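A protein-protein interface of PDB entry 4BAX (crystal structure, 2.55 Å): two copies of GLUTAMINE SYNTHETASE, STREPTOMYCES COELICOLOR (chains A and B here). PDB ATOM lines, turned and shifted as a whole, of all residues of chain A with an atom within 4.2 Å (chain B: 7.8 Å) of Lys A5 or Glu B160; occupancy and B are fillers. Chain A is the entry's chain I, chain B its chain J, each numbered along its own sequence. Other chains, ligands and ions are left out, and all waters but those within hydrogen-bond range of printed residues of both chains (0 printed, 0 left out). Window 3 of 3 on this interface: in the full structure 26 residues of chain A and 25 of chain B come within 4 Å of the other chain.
The side-chain amino group (NZ) of Lys A5 lies within salt-bridge range of the side-chain carboxylate (OE1) of Glu B160, at 3.1 Å. NH2 of Arg A70 lies within salt-bridge range of OE2 of Glu B156, 2.9 Å away.
The backbone NH (N) of Lys A5 is in hydrogen-bond range of the side-chain carboxylate (OD1) of Asp A74, at 2.9 Å. O of Lys A5 lies within hydrogen-bond range of N of Ile A75 (3.0 Å). OE1 of Glu A7 is in salt-bridge range of NH1 of Arg A70 (2.9 Å).
Among the printed residues, pairs that only touch across the chains: Ile A26 with Ile B169, Lys A5 with Leu B163, Lys A5 with Leu B159 and Arg A70 with Leu B159.
Printed residues of chain B within 4 Å of Ile A26: Ile B169. Pro B68 touches none of the printed residues of chain A. Printed residues of chain A within 4 Å of Glu B156: Arg A70 (2.9 Å). Of the printed residues of chain A, Leu B159 touches Lys A5 (3.8 Å) and Arg A70 (3.98 Å). Lys B164 touches none of the printed residues of chain A. The nearest residue of chain B that does not touch Lys A5 is Glu B156 (5.2 Å).
Of the 18 printed residues of chain B, 5 touch a printed residue of chain A. Of the 9 printed residues of chain A, 3 touch a printed residue of chain B. Among the printed residues, Asp or Glu carboxylates within 4 Å of a Lys or Arg side-chain nitrogen of the other chain: Lys A5 with Glu B160 and Arg A70 with Glu B156.
No position is printed for both chains. Of the 6 pairs that touch across the chains among the printed residues, none has its exchanged pair printed and touching as well.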
ATOM      1  N   PHE A   4      13.844  22.965 -15.216  1.00  0.00           N
ATOM      2  CA  PHE A   4      13.342  21.798 -14.508  1.00  0.00           C
ATOM      3  C   PHE A   4      14.227  21.489 -13.318  1.00  0.00           C
ATOM      4  O   PHE A   4      15.375  21.923 -13.229  1.00  0.00           O
ATOM      5  CB  PHE A   4      13.172  20.596 -15.459  1.00  0.00           C
ATOM      6  CG  PHE A   4      14.464  20.034 -15.978  1.00  0.00           C
ATOM      7  CD1 PHE A   4      15.101  20.629 -17.070  1.00  0.00           C
ATOM      8  CD2 PHE A   4      15.063  18.935 -15.376  1.00  0.00           C
ATOM      9  CE1 PHE A   4      16.310  20.129 -17.564  1.00  0.00           C
ATOM     10  CE2 PHE A   4      16.277  18.425 -15.865  1.00  0.00           C
ATOM     11  CZ  PHE A   4      16.899  19.024 -16.956  1.00  0.00           C
ATOM     12  N   LYS A   5      13.675  20.741 -12.388  1.00  0.00           N
ATOM     13  CA  LYS A   5      14.397  20.403 -11.182  1.00  0.00           C
ATOM     14  C   LYS A   5      15.098  19.064 -11.283  1.00  0.00           C
ATOM     15  O   LYS A   5      14.523  18.081 -11.758  1.00  0.00           O
ATOM     16  CB  LYS A   5      13.419  20.401 -10.016  1.00  0.00           C
ATOM     17  CG  LYS A   5      12.907  21.805  -9.738  1.00  0.00           C
ATOM     18  CD  LYS A   5      12.003  21.845  -8.533  1.00  0.00           C
ATOM     19  CE  LYS A   5      10.561  21.797  -8.924  1.00  0.00           C
ATOM     20  NZ  LYS A   5      10.077  23.202  -8.979  1.00  0.00           N
ATOM     21  N   ALA A   6      16.349  19.037 -10.831  1.00  0.00           N
ATOM     22  CA  ALA A   6      17.101  17.796 -10.779  1.00  0.00           C
ATOM     23  C   ALA A   6      17.550  17.552  -9.343  1.00  0.00           C
ATOM     24  O   ALA A   6      18.249  18.375  -8.737  1.00  0.00           O
ATOM     25  CB  ALA A   6      18.303  17.859 -11.712  1.00  0.00           C
ATOM     26  N   GLU A   7      17.123  16.416  -8.802  1.00  0.00           N
ATOM     27  CA  GLU A   7      17.506  16.021  -7.451  1.00  0.00           C
ATOM     28  C   GLU A   7      18.687  15.062  -7.554  1.00  0.00           C
ATOM     29  O   GLU A   7      18.536  13.904  -8.001  1.00  0.00           O
ATOM     30  CB  GLU A   7      16.325  15.369  -6.707  1.00  0.00           C
ATOM     31  CG  GLU A   7      16.535  15.202  -5.216  1.00  0.00           C
ATOM     32  CD  GLU A   7      16.405  16.509  -4.472  1.00  0.00           C
ATOM     33  OE1 GLU A   7      16.078  17.515  -5.144  1.00  0.00           O
ATOM     34  OE2 GLU A   7      16.672  16.543  -3.238  1.00  0.00           O
ATOM     35  N   LYS A  25      19.118  20.818  -7.887  1.00  0.00           N
ATOM     36  CA  LYS A  25      19.776  21.687  -8.841  1.00  0.00           C
ATOM     37  C   LYS A  25      18.743  22.210  -9.835  1.00  0.00           C
ATOM     38  O   LYS A  25      17.888  21.452 -10.330  1.00  0.00           O
ATOM     39  CB  LYS A  25      20.848  20.895  -9.588  1.00  0.00           C
ATOM     40  CG  LYS A  25      21.710  21.720 -10.536  1.00  0.00           C
ATOM     41  CD  LYS A  25      22.945  20.933 -10.967  1.00  0.00           C
ATOM     42  CE  LYS A  25      23.916  21.825 -11.701  1.00  0.00           C
ATOM     43  NZ  LYS A  25      24.920  22.310 -10.724  1.00  0.00           N
ATOM     44  N   ILE A  26      18.789  23.496 -10.129  1.00  0.00           N
ATOM     45  CA  ILE A  26      17.852  24.002 -11.114  1.00  0.00           C
ATOM     46  C   ILE A  26      18.567  24.086 -12.455  1.00  0.00           C
ATOM     47  O   ILE A  26      19.586  24.773 -12.596  1.00  0.00           O
ATOM     48  CB  ILE A  26      17.324  25.382 -10.717  1.00  0.00           C
ATOM     49  CG1 ILE A  26      16.713  25.311  -9.308  1.00  0.00           C
ATOM     50  CG2 ILE A  26      16.322  25.903 -11.734  1.00  0.00           C
ATOM     51  CD1 ILE A  26      15.496  24.438  -9.183  1.00  0.00           C
ATOM     52  N   ARG A  70       7.701  15.461  -7.476  1.00  0.00           N
ATOM     53  CA  ARG A  70       7.605  16.793  -8.064  1.00  0.00           C
ATOM     54  C   ARG A  70       6.723  16.767  -9.299  1.00  0.00           C
ATOM     55  O   ARG A  70       5.980  17.707  -9.564  1.00  0.00           O
ATOM     56  CB  ARG A  70       8.990  17.337  -8.386  1.00  0.00           C
ATOM     57  CG  ARG A  70       9.564  18.171  -7.260  1.00  0.00           C
ATOM     58  CD  ARG A  70      11.069  18.258  -7.379  1.00  0.00           C
ATOM     59  NE  ARG A  70      11.635  19.007  -6.267  1.00  0.00           N
ATOM     60  CZ  ARG A  70      12.939  19.116  -6.022  1.00  0.00           C
ATOM     61  NH1 ARG A  70      13.831  18.475  -6.776  1.00  0.00           N
ATOM     62  NH2 ARG A  70      13.358  19.824  -4.975  1.00  0.00           N
ATOM     63  N   ASP A  74      10.403  17.237 -13.893  1.00  0.00           N
ATOM     64  CA  ASP A  74      11.427  17.122 -12.856  1.00  0.00           C
ATOM     65  C   ASP A  74      11.941  15.675 -12.784  1.00  0.00           C
ATOM     66  O   ASP A  74      11.215  14.740 -13.129  1.00  0.00           O
ATOM     67  CB  ASP A  74      10.858  17.597 -11.518  1.00  0.00           C
ATOM     68  CG  ASP A  74      10.418  19.066 -11.564  1.00  0.00           C
ATOM     69  OD1 ASP A  74      10.929  19.832 -12.413  1.00  0.00           O
ATOM     70  OD2 ASP A  74       9.506  19.447 -10.801  1.00  0.00           O
ATOM     71  N   ILE A  75      13.208  15.507 -12.402  1.00  0.00           N
ATOM     72  CA  ILE A  75      13.857  14.193 -12.459  1.00  0.00           C
ATOM     73  C   ILE A  75      14.712  13.892 -11.215  1.00  0.00           C
ATOM     74  O   ILE A  75      15.115  14.805 -10.470  1.00  0.00           O
ATOM     75  CB  ILE A  75      14.733  14.057 -13.754  1.00  0.00           C
ATOM     76  CG1 ILE A  75      15.708  15.227 -13.948  1.00  0.00           C
ATOM     77  CG2 ILE A  75      13.866  13.945 -14.992  1.00  0.00           C
ATOM     78  CD1 ILE A  75      17.120  14.808 -14.431  1.00  0.00           C
ATOM     79  N   PRO B  68       3.242  34.658  -7.055  1.00  0.00           N
ATOM     80  CA  PRO B  68       3.006  33.223  -7.239  1.00  0.00           C
ATOM     81  C   PRO B  68       1.943  32.675  -6.290  1.00  0.00           C
ATOM     82  O   PRO B  68       1.270  31.686  -6.596  1.00  0.00           O
ATOM     83  CB  PRO B  68       4.375  32.609  -6.938  1.00  0.00           C
ATOM     84  CG  PRO B  68       4.975  33.563  -5.948  1.00  0.00           C
ATOM     85  CD  PRO B  68       4.518  34.931  -6.372  1.00  0.00           C
ATOM     86  N   VAL B 154       7.581  23.244   3.375  1.00  0.00           N
ATOM     87  CA  VAL B 154       7.764  24.684   3.266  1.00  0.00           C
ATOM     88  C   VAL B 154       8.817  25.035   2.226  1.00  0.00           C
ATOM     89  O   VAL B 154       8.601  25.907   1.367  1.00  0.00           O
ATOM     90  CB  VAL B 154       8.193  25.292   4.612  1.00  0.00           C
ATOM     91  CG1 VAL B 154       8.195  26.807   4.513  1.00  0.00           C
ATOM     92  CG2 VAL B 154       7.262  24.807   5.746  1.00  0.00           C
ATOM     93  N   VAL B 155       9.942  24.320   2.289  1.00  0.00           N
ATOM     94  CA  VAL B 155      11.062  24.587   1.394  1.00  0.00           C
ATOM     95  C   VAL B 155      10.622  24.363  -0.050  1.00  0.00           C
ATOM     96  O   VAL B 155      10.919  25.192  -0.911  1.00  0.00           O
ATOM     97  CB  VAL B 155      12.283  23.692   1.725  1.00  0.00           C
ATOM     98  CG1 VAL B 155      13.380  23.878   0.679  1.00  0.00           C
ATOM     99  CG2 VAL B 155      12.827  23.991   3.117  1.00  0.00           C
ATOM    100  N   GLU B 156       9.867  23.286  -0.300  1.00  0.00           N
ATOM    101  CA  GLU B 156       9.367  22.985  -1.655  1.00  0.00           C
ATOM    102  C   GLU B 156       8.368  24.000  -2.153  1.00  0.00           C
ATOM    103  O   GLU B 156       8.417  24.388  -3.329  1.00  0.00           O
ATOM    104  CB  GLU B 156       8.738  21.582  -1.730  1.00  0.00           C
ATOM    105  CG  GLU B 156       9.690  20.410  -1.537  1.00  0.00           C
ATOM    106  CD  GLU B 156      10.472  20.071  -2.789  1.00  0.00           C
ATOM    107  OE1 GLU B 156      10.023  20.418  -3.903  1.00  0.00           O
ATOM    108  OE2 GLU B 156      11.569  19.500  -2.661  1.00  0.00           O
ATOM    109  N   ALA B 157       7.471  24.434  -1.262  1.00  0.00           N
ATOM    110  CA  ALA B 157       6.486  25.445  -1.626  1.00  0.00           C
ATOM    111  C   ALA B 157       7.189  26.761  -1.960  1.00  0.00           C
ATOM    112  O   ALA B 157       6.889  27.355  -3.014  1.00  0.00           O
ATOM    113  CB  ALA B 157       5.465  25.635  -0.500  1.00  0.00           C
ATOM    114  N   HIS B 158       8.211  27.115  -1.159  1.00  0.00           N
ATOM    115  CA  HIS B 158       9.000  28.351  -1.354  1.00  0.00           C
ATOM    116  C   HIS B 158       9.784  28.305  -2.651  1.00  0.00           C
ATOM    117  O   HIS B 158       9.860  29.288  -3.390  1.00  0.00           O
ATOM    118  CB  HIS B 158       9.948  28.602  -0.173  1.00  0.00           C
ATOM    119  CG  HIS B 158      10.920  29.722  -0.402  1.00  0.00           C
ATOM    120  ND1 HIS B 158      12.265  29.516  -0.644  1.00  0.00           N
ATOM    121  CD2 HIS B 158      10.745  31.066  -0.405  1.00  0.00           C
ATOM    122  CE1 HIS B 158      12.871  30.683  -0.799  1.00  0.00           C
ATOM    123  NE2 HIS B 158      11.971  31.639  -0.655  1.00  0.00           N
ATOM    124  N   LEU B 159      10.372  27.156  -2.933  1.00  0.00           N
ATOM    125  CA  LEU B 159      11.124  27.028  -4.163  1.00  0.00           C
ATOM    126  C   LEU B 159      10.200  27.199  -5.380  1.00  0.00           C
ATOM    127  O   LEU B 159      10.498  27.992  -6.293  1.00  0.00           O
ATOM    128  CB  LEU B 159      11.895  25.702  -4.190  1.00  0.00           C
ATOM    129  CG  LEU B 159      12.537  25.222  -5.494  1.00  0.00           C
ATOM    130  CD1 LEU B 159      13.747  26.063  -5.859  1.00  0.00           C
ATOM    131  CD2 LEU B 159      12.921  23.759  -5.373  1.00  0.00           C
ATOM    132  N   GLU B 160       9.042  26.545  -5.352  1.00  0.00           N
ATOM    133  CA  GLU B 160       8.093  26.686  -6.443  1.00  0.00           C
ATOM    134  C   GLU B 160       7.614  28.134  -6.597  1.00  0.00           C
ATOM    135  O   GLU B 160       7.530  28.644  -7.718  1.00  0.00           O
ATOM    136  CB  GLU B 160       6.901  25.738  -6.230  1.00  0.00           C
ATOM    137  CG  GLU B 160       5.830  25.733  -7.319  1.00  0.00           C
ATOM    138  CD  GLU B 160       6.330  25.240  -8.679  1.00  0.00           C
ATOM    139  OE1 GLU B 160       7.524  24.880  -8.807  1.00  0.00           O
ATOM    140  OE2 GLU B 160       5.528  25.246  -9.643  1.00  0.00           O
ATOM    141  N   ASN B 161       7.414  28.827  -5.479  1.00  0.00           N
ATOM    142  CA  ASN B 161       7.003  30.232  -5.517  1.00  0.00           C
ATOM    143  C   ASN B 161       8.086  31.134  -6.129  1.00  0.00           C
ATOM    144  O   ASN B 161       7.788  32.021  -6.935  1.00  0.00           O
ATOM    145  CB  ASN B 161       6.630  30.715  -4.108  1.00  0.00           C
ATOM    146  CG  ASN B 161       5.195  30.314  -3.707  1.00  0.00           C
ATOM    147  OD1 ASN B 161       4.367  29.980  -4.562  1.00  0.00           O
ATOM    148  ND2 ASN B 161       4.908  30.344  -2.403  1.00  0.00           N
ATOM    149  N   CYS B 162       9.343  30.890  -5.781  1.00  0.00           N
ATOM    150  CA  CYS B 162      10.441  31.686  -6.326  1.00  0.00           C
ATOM    151  C   CYS B 162      10.585  31.536  -7.852  1.00  0.00           C
ATOM    152  O   CYS B 162      10.764  32.529  -8.574  1.00  0.00           O
ATOM    153  CB  CYS B 162      11.740  31.295  -5.644  1.00  0.00           C
ATOM    154  SG  CYS B 162      11.863  31.939  -3.962  1.00  0.00           S
ATOM    155  N   LEU B 163      10.460  30.298  -8.340  1.00  0.00           N
ATOM    156  CA  LEU B 163      10.570  30.019  -9.774  1.00  0.00           C
ATOM    157  C   LEU B 163       9.423  30.610 -10.569  1.00  0.00           C
ATOM    158  O   LEU B 163       9.631  31.191 -11.629  1.00  0.00           O
ATOM    159  CB  LEU B 163      10.693  28.512 -10.036  1.00  0.00           C
ATOM    160  CG  LEU B 163      11.944  27.860  -9.460  1.00  0.00           C
ATOM    161  CD1 LEU B 163      11.896  26.358  -9.596  1.00  0.00           C
ATOM    162  CD2 LEU B 163      13.162  28.419 -10.170  1.00  0.00           C
ATOM    163  N   LYS B 164       8.226  30.516 -10.007  1.00  0.00           N
ATOM    164  CA  LYS B 164       7.043  31.109 -10.589  1.00  0.00           C
ATOM    165  C   LYS B 164       7.169  32.638 -10.645  1.00  0.00           C
ATOM    166  O   LYS B 164       6.648  33.291 -11.552  1.00  0.00           O
ATOM    167  CB  LYS B 164       5.821  30.710  -9.781  1.00  0.00           C
ATOM    168  CG  LYS B 164       4.982  29.721 -10.507  1.00  0.00           C
ATOM    169  CD  LYS B 164       4.603  28.583  -9.595  1.00  0.00           C
ATOM    170  CE  LYS B 164       3.626  29.096  -8.548  1.00  0.00           C
ATOM    171  NZ  LYS B 164       2.361  28.305  -8.497  1.00  0.00           N
ATOM    172  N   ALA B 165       7.848  33.206  -9.658  1.00  0.00           N
ATOM    173  CA  ALA B 165       8.145  34.636  -9.664  1.00  0.00           C
ATOM    174  C   ALA B 165       9.205  35.007 -10.714  1.00  0.00           C
ATOM    175  O   ALA B 165       9.339  36.177 -11.065  1.00  0.00           O
ATOM    176  CB  ALA B 165       8.584  35.090  -8.273  1.00  0.00           C
ATOM    177  N   GLY B 166       9.904  34.002 -11.249  1.00  0.00           N
ATOM    178  CA  GLY B 166      10.938  34.198 -12.252  1.00  0.00           C
ATOM    179  C   GLY B 166      12.317  34.463 -11.648  1.00  0.00           C
ATOM    180  O   GLY B 166      13.246  34.844 -12.366  1.00  0.00           O
ATOM    181  N   ILE B 169      16.905  31.041  -9.174  1.00  0.00           N
ATOM    182  CA  ILE B 169      17.312  30.107  -8.154  1.00  0.00           C
ATOM    183  C   ILE B 169      18.052  28.988  -8.875  1.00  0.00           C
ATOM    184  O   ILE B 169      17.546  28.423  -9.853  1.00  0.00           O
ATOM    185  CB  ILE B 169      16.083  29.522  -7.427  1.00  0.00           C
ATOM    186  CG1 ILE B 169      15.153  30.646  -6.966  1.00  0.00           C
ATOM    187  CG2 ILE B 169      16.499  28.616  -6.263  1.00  0.00           C
ATOM    188  CD1 ILE B 169      15.780  31.551  -5.938  1.00  0.00           C
ATOM    189  N   ILE B 172      18.680  24.389  -4.108  1.00  0.00           N
ATOM    190  CA  ILE B 172      18.376  24.443  -2.694  1.00  0.00           C
ATOM    191  C   ILE B 172      18.981  23.211  -2.049  1.00  0.00           C
ATOM    192  O   ILE B 172      19.208  22.199  -2.737  1.00  0.00           O
ATOM    193  CB  ILE B 172      16.856  24.481  -2.425  1.00  0.00           C
ATOM    194  CG1 ILE B 172      16.199  23.273  -3.101  1.00  0.00           C
ATOM    195  CG2 ILE B 172      16.223  25.749  -3.011  1.00  0.00           C
ATOM    196  CD1 ILE B 172      15.000  22.680  -2.364  1.00  0.00           C
ATOM    197  N   LEU B 203       9.306  35.958   0.254  1.00  0.00           N
ATOM    198  CA  LEU B 203       8.541  34.773  -0.119  1.00  0.00           C
ATOM    199  C   LEU B 203       8.716  33.657   0.929  1.00  0.00           C
ATOM    200  O   LEU B 203       7.773  32.925   1.221  1.00  0.00           O
ATOM    201  CB  LEU B 203       8.942  34.301  -1.525  1.00  0.00           C
ATOM    202  CG  LEU B 203       8.326  35.123  -2.679  1.00  0.00           C
ATOM    203  CD1 LEU B 203       8.926  34.766  -4.037  1.00  0.00           C
ATOM    204  CD2 LEU B 203       6.817  34.970  -2.734  1.00  0.00           C
ATOM    205  N   THR B 207       5.543  32.419   2.730  1.00  0.00           N
ATOM    206  CA  THR B 207       5.147  31.031   2.438  1.00  0.00           C
ATOM    207  C   THR B 207       4.995  30.249   3.723  1.00  0.00           C
ATOM    208  O   THR B 207       4.056  29.455   3.860  1.00  0.00           O
ATOM    209  CB  THR B 207       6.179  30.315   1.504  1.00  0.00           C
ATOM    210  OG1 THR B 207       6.268  31.015   0.247  1.00  0.00           O
ATOM    211  CG2 THR B 207       5.765  28.883   1.202  1.00  0.00           C
